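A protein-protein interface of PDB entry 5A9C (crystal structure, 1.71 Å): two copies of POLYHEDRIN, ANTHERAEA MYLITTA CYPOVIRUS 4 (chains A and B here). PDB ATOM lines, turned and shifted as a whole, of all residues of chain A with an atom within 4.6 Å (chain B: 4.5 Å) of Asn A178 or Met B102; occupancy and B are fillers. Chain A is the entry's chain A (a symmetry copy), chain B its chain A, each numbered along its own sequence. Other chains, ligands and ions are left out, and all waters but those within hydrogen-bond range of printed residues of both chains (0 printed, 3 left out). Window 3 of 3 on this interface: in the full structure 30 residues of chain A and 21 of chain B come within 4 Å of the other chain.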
ATOM      1  N   ALA A  53     -17.543  -4.984  22.299  1.00  0.00           N
ATOM      2  CA  ALA A  53     -18.621  -4.297  21.605  1.00  0.00           C
ATOM      3  C   ALA A  53     -18.196  -3.825  20.221  1.00  0.00           C
ATOM      4  O   ALA A  53     -17.122  -3.248  20.051  1.00  0.00           O
ATOM      5  CB  ALA A  53     -19.120  -3.120  22.438  1.00  0.00           C
ATOM      6  N   PHE A  54     -19.042  -4.099  19.234  1.00  0.00           N
ATOM      7  CA  PHE A  54     -18.884  -3.538  17.900  1.00  0.00           C
ATOM      8  C   PHE A  54     -19.940  -2.457  17.718  1.00  0.00           C
ATOM      9  O   PHE A  54     -21.120  -2.749  17.516  1.00  0.00           O
ATOM     10  CB  PHE A  54     -19.012  -4.629  16.836  1.00  0.00           C
ATOM     11  CG  PHE A  54     -18.019  -5.743  17.001  1.00  0.00           C
ATOM     12  CD1 PHE A  54     -18.282  -6.801  17.857  1.00  0.00           C
ATOM     13  CD2 PHE A  54     -16.807  -5.717  16.330  1.00  0.00           C
ATOM     14  CE1 PHE A  54     -17.365  -7.820  18.024  1.00  0.00           C
ATOM     15  CE2 PHE A  54     -15.888  -6.734  16.494  1.00  0.00           C
ATOM     16  CZ  PHE A  54     -16.166  -7.786  17.342  1.00  0.00           C
ATOM     17  N   ASP A  55     -19.498  -1.207  17.803  1.00  0.00           N
ATOM     18  CA  ASP A  55     -20.385  -0.052  17.890  1.00  0.00           C
ATOM     19  C   ASP A  55     -20.406   0.726  16.577  1.00  0.00           C
ATOM     20  O   ASP A  55     -19.399   1.315  16.182  1.00  0.00           O
ATOM     21  CB  ASP A  55     -19.898   0.851  19.021  1.00  0.00           C
ATOM     22  CG  ASP A  55     -20.881   1.949  19.368  1.00  0.00           C
ATOM     23  OD1 ASP A  55     -21.800   2.216  18.571  1.00  0.00           O
ATOM     24  OD2 ASP A  55     -20.714   2.550  20.448  1.00  0.00           O
ATOM     25  N   CYS A 176     -19.447   4.432  10.824  1.00  0.00           N
ATOM     26  CA  CYS A 176     -18.316   4.642  11.718  1.00  0.00           C
ATOM     27  C   CYS A 176     -18.288   3.589  12.818  1.00  0.00           C
ATOM     28  O   CYS A 176     -19.011   3.702  13.808  1.00  0.00           O
ATOM     29  CB  CYS A 176     -18.382   6.038  12.331  1.00  0.00           C
ATOM     30  SG  CYS A 176     -18.459   7.352  11.113  1.00  0.00           S
ATOM     31  N   PRO A 177     -17.459   2.553  12.636  1.00  0.00           N
ATOM     32  CA  PRO A 177     -17.324   1.450  13.590  1.00  0.00           C
ATOM     33  C   PRO A 177     -16.290   1.722  14.673  1.00  0.00           C
ATOM     34  O   PRO A 177     -15.247   2.323  14.408  1.00  0.00           O
ATOM     35  CB  PRO A 177     -16.834   0.284  12.713  1.00  0.00           C
ATOM     36  CG  PRO A 177     -16.885   0.784  11.286  1.00  0.00           C
ATOM     37  CD  PRO A 177     -16.752   2.264  11.380  1.00  0.00           C
ATOM     38  N   ASN A 178     -16.590   1.282  15.889  1.00  0.00           N
ATOM     39  CA  ASN A 178     -15.598   1.206  16.951  1.00  0.00           C
ATOM     40  C   ASN A 178     -15.679  -0.136  17.658  1.00  0.00           C
ATOM     41  O   ASN A 178     -16.765  -0.682  17.860  1.00  0.00           O
ATOM     42  CB  ASN A 178     -15.764   2.344  17.956  1.00  0.00           C
ATOM     43  CG  ASN A 178     -14.930   3.554  17.601  1.00  0.00           C
ATOM     44  OD1 ASN A 178     -13.706   3.541  17.749  1.00  0.00           O
ATOM     45  ND2 ASN A 178     -15.586   4.607  17.131  1.00  0.00           N
ATOM     46  N   VAL A 179     -14.523  -0.675  18.023  1.00  0.00           N
ATOM     47  CA  VAL A 179     -14.478  -1.913  18.780  1.00  0.00           C
ATOM     48  C   VAL A 179     -14.013  -1.588  20.188  1.00  0.00           C
ATOM     49  O   VAL A 179     -12.954  -0.990  20.380  1.00  0.00           O
ATOM     50  CB  VAL A 179     -13.534  -2.943  18.137  1.00  0.00           C
ATOM     51  CG1 VAL A 179     -13.613  -4.264  18.881  1.00  0.00           C
ATOM     52  CG2 VAL A 179     -13.887  -3.133  16.671  1.00  0.00           C
ATOM     53  N   ILE A 180     -14.821  -1.967  21.171  1.00  0.00           N
ATOM     54  CA  ILE A 180     -14.546  -1.623  22.556  1.00  0.00           C
ATOM     55  C   ILE A 180     -14.510  -2.867  23.429  1.00  0.00           C
ATOM     56  O   ILE A 180     -15.412  -3.705  23.372  1.00  0.00           O
ATOM     57  CB  ILE A 180     -15.602  -0.648  23.096  1.00  0.00           C
ATOM     58  CG1 ILE A 180     -15.743   0.539  22.141  1.00  0.00           C
ATOM     59  CG2 ILE A 180     -15.238  -0.183  24.503  1.00  0.00           C
ATOM     60  CD1 ILE A 180     -16.829   1.493  22.518  1.00  0.00           C
ATOM     61  N   PHE B  65     -13.780   6.909   6.852  1.00  0.00           N
ATOM     62  CA  PHE B  65     -13.758   7.117   8.293  1.00  0.00           C
ATOM     63  C   PHE B  65     -12.508   6.475   8.860  1.00  0.00           C
ATOM     64  O   PHE B  65     -12.365   5.253   8.854  1.00  0.00           O
ATOM     65  CB  PHE B  65     -14.998   6.540   8.981  1.00  0.00           C
ATOM     66  CG  PHE B  65     -14.915   6.562  10.491  1.00  0.00           C
ATOM     67  CD1 PHE B  65     -15.079   7.745  11.191  1.00  0.00           C
ATOM     68  CD2 PHE B  65     -14.659   5.401  11.205  1.00  0.00           C
ATOM     69  CE1 PHE B  65     -14.997   7.772  12.574  1.00  0.00           C
ATOM     70  CE2 PHE B  65     -14.579   5.422  12.591  1.00  0.00           C
ATOM     71  CZ  PHE B  65     -14.748   6.608  13.275  1.00  0.00           C
ATOM     72  N   TRP B  68      -9.650   6.049  15.581  1.00  0.00           N
ATOM     73  CA  TRP B  68      -8.553   6.575  16.385  1.00  0.00           C
ATOM     74  C   TRP B  68      -7.346   5.638  16.442  1.00  0.00           C
ATOM     75  O   TRP B  68      -6.208   6.091  16.575  1.00  0.00           O
ATOM     76  CB  TRP B  68      -9.033   6.931  17.798  1.00  0.00           C
ATOM     77  CG  TRP B  68      -9.376   5.748  18.645  1.00  0.00           C
ATOM     78  CD1 TRP B  68     -10.586   5.121  18.729  1.00  0.00           C
ATOM     79  CD2 TRP B  68      -8.499   5.050  19.536  1.00  0.00           C
ATOM     80  NE1 TRP B  68     -10.515   4.073  19.616  1.00  0.00           N
ATOM     81  CE2 TRP B  68      -9.244   4.008  20.125  1.00  0.00           C
ATOM     82  CE3 TRP B  68      -7.156   5.204  19.892  1.00  0.00           C
ATOM     83  CZ2 TRP B  68      -8.690   3.125  21.050  1.00  0.00           C
ATOM     84  CZ3 TRP B  68      -6.607   4.327  20.811  1.00  0.00           C
ATOM     85  CH2 TRP B  68      -7.374   3.300  21.378  1.00  0.00           C
ATOM     86  N   ARG B  69      -7.588   4.337  16.334  1.00  0.00           N
ATOM     87  CA  ARG B  69      -6.493   3.374  16.388  1.00  0.00           C
ATOM     88  C   ARG B  69      -5.728   3.330  15.065  1.00  0.00           C
ATOM     89  O   ARG B  69      -4.513   3.137  15.048  1.00  0.00           O
ATOM     90  CB  ARG B  69      -6.995   1.983  16.803  1.00  0.00           C
ATOM     91  CG  ARG B  69      -7.881   1.285  15.783  1.00  0.00           C
ATOM     92  CD  ARG B  69      -8.716   0.184  16.429  1.00  0.00           C
ATOM     93  NE  ARG B  69      -9.856   0.718  17.172  1.00  0.00           N
ATOM     94  CZ  ARG B  69     -11.129   0.553  16.819  1.00  0.00           C
ATOM     95  NH1 ARG B  69     -11.436  -0.146  15.736  1.00  0.00           N
ATOM     96  NH2 ARG B  69     -12.097   1.075  17.561  1.00  0.00           N
ATOM     97  N   THR B 100     -14.377  14.240  13.818  1.00  0.00           N
ATOM     98  CA  THR B 100     -15.415  13.798  14.739  1.00  0.00           C
ATOM     99  C   THR B 100     -14.766  13.294  16.025  1.00  0.00           C
ATOM    100  O   THR B 100     -13.538  13.314  16.156  1.00  0.00           O
ATOM    101  CB  THR B 100     -16.283  12.697  14.099  1.00  0.00           C
ATOM    102  OG1 THR B 100     -15.457  11.849  13.291  1.00  0.00           O
ATOM    103  CG2 THR B 100     -17.357  13.316  13.207  1.00  0.00           C
ATOM    104  N   ASN B 101     -15.579  12.861  16.981  1.00  0.00           N
ATOM    105  CA  ASN B 101     -15.035  12.334  18.229  1.00  0.00           C
ATOM    106  C   ASN B 101     -14.627  10.873  18.079  1.00  0.00           C
ATOM    107  O   ASN B 101     -14.673  10.322  16.980  1.00  0.00           O
ATOM    108  CB  ASN B 101     -15.999  12.544  19.408  1.00  0.00           C
ATOM    109  CG  ASN B 101     -17.212  11.625  19.359  1.00  0.00           C
ATOM    110  OD1 ASN B 101     -17.319  10.744  18.501  1.00  0.00           O
ATOM    111  ND2 ASN B 101     -18.127  11.820  20.298  1.00  0.00           N
ATOM    112  N   MET B 102     -14.221  10.248  19.180  1.00  0.00           N
ATOM    113  CA  MET B 102     -13.693   8.891  19.117  1.00  0.00           C
ATOM    114  C   MET B 102     -14.692   7.904  18.517  1.00  0.00           C
ATOM    115  O   MET B 102     -14.306   6.847  18.014  1.00  0.00           O
ATOM    116  CB  MET B 102     -13.244   8.417  20.502  1.00  0.00           C
ATOM    117  CG  MET B 102     -14.379   8.141  21.465  1.00  0.00           C
ATOM    118  SD  MET B 102     -13.797   7.566  23.074  1.00  0.00           S
ATOM    119  CE  MET B 102     -12.860   8.990  23.622  1.00  0.00           C
ATOM    120  N   HIS B 103     -15.975   8.254  18.565  1.00  0.00           N
ATOM    121  CA  HIS B 103     -17.031   7.367  18.084  1.00  0.00           C
ATOM    122  C   HIS B 103     -17.457   7.688  16.655  1.00  0.00           C
ATOM    123  O   HIS B 103     -18.303   6.997  16.082  1.00  0.00           O
ATOM    124  CB  HIS B 103     -18.246   7.432  19.014  1.00  0.00           C
ATOM    125  CG  HIS B 103     -17.927   7.110  20.442  1.00  0.00           C
ATOM    126  ND1 HIS B 103     -17.908   5.822  20.929  1.00  0.00           N
ATOM    127  CD2 HIS B 103     -17.607   7.912  21.486  1.00  0.00           C
ATOM    128  CE1 HIS B 103     -17.591   5.842  22.212  1.00  0.00           C
ATOM    129  NE2 HIS B 103     -17.404   7.098  22.573  1.00  0.00           N
ATOM    130  N   GLY B 104     -16.870   8.732  16.080  1.00  0.00           N
ATOM    131  CA  GLY B 104     -17.230   9.160  14.741  1.00  0.00           C
ATOM    132  C   GLY B 104     -18.433  10.086  14.741  1.00  0.00           C
ATOM    133  O   GLY B 104     -19.091  10.273  13.715  1.00  0.00           O
ATOM    134  N   HIS B 143      -7.742  11.360  20.194  1.00  0.00           N
ATOM    135  CA  HIS B 143      -8.956  10.569  20.003  1.00  0.00           C
ATOM    136  C   HIS B 143      -9.916  11.105  18.940  1.00  0.00           C
ATOM    137  O   HIS B 143     -10.916  10.458  18.625  1.00  0.00           O
ATOM    138  CB  HIS B 143      -9.679  10.345  21.333  1.00  0.00           C
ATOM    139  CG  HIS B 143      -8.911   9.497  22.298  1.00  0.00           C
ATOM    140  ND1 HIS B 143      -7.685   8.946  21.988  1.00  0.00           N
ATOM    141  CD2 HIS B 143      -9.191   9.103  23.561  1.00  0.00           C
ATOM    142  CE1 HIS B 143      -7.245   8.250  23.021  1.00  0.00           C
ATOM    143  NE2 HIS B 143      -8.139   8.330  23.989  1.00  0.00           N
ATOM    144  N   THR B 145     -11.409  11.616  15.345  1.00  0.00           N
ATOM    145  CA  THR B 145     -11.416  10.766  14.162  1.00  0.00           C
ATOM    146  C   THR B 145     -11.606  11.636  12.928  1.00  0.00           C
ATOM    147  O   THR B 145     -11.947  12.810  13.046  1.00  0.00           O
ATOM    148  CB  THR B 145     -12.508   9.677  14.224  1.00  0.00           C
ATOM    149  OG1 THR B 145     -13.749  10.260  14.639  1.00  0.00           O
ATOM    150  CG2 THR B 145     -12.111   8.575  15.201  1.00  0.00           C
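No position is printed for both chains.
Printed residues of chain B that touch a printed residue of chain A: Phe B65, Trp B68, Arg B69, Met B102, His B103 and Gly B104. Hydrophobic or aromatic side chains of chain B within 4 Å of the printed part of chain A: Phe B65 and Trp B68. Of the 8 printed residues of chain A, 4 touch a printed residue of chain B. Hydrophobic or aromatic side chains of chain A within 4 Å of the printed part of chain B: Pro A177 and Val A179. Among the printed residues, 9 pairs touch across the chains. Among the printed residues, no Asp or Glu carboxylate lies within 4 Å of a Lys or Arg side-chain nitrogen of the other chain.
The side-chain sulfur of Met B102 lies close to a ring nitrogen (NE2) of His B103. N of Met B102 lies close to O of His B143. The side-chain amide oxygen of Asn B101 is in hydrogen-bond range of the backbone NH of His B103 (2.8 Å). The backbone NH (N) of Asp A55 is in hydrogen-bond range of the backbone carbonyl oxygen (O) of Asn A178, 2.8 Å away. The backbone NH of Gly B104 is in hydrogen-bond range of the side-chain amide oxygen of Asn B101 (3.2 Å).
NH2 of Arg B69 sits at hydrogen-bond distance from OD1 of Asn A178, 3.0 Å away. ND2 of Asn A178 is in hydrogen-bond range of O of Met B102 (2.7 Å). The backbone NH of Val A179 lies close to the guanidinium group of Arg B69.
Printed residues of chain B within 4 Å of Pro A177: Phe B65 (3.7 Å). Asn A178 touches just these residues of chain B: Trp B68, Arg B69, Met B102 and His B103. Printed residues of chain A within 4 Å of Phe B65: Cys A176 and Pro A177. Of the printed residues of chain A, Arg B69 touches Asn A178 (3.0 Å) and Val A179 (3.0 Å). Met B102 touches one residue of chain A. Of the printed residues of chain A, Gly B104 touches Cys A176 (3.96 Å). The nearest printed residue of chain B that does not touch Asn A178 is Phe B65 (4.4 Å).
Phe B65 touches Cys A176. Cys A176 touches His B103 (CB to O, 3.9 Å). Gly B104 touches Cys A176. Pro A177 touches Phe B65 (O to CE2, 3.7 Å). CD1 of Trp B68 touches OD1 of Asn A178, 3.6 Å away. Asn A178 touches His B103 (ND2 to CA, 3.3 Å).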
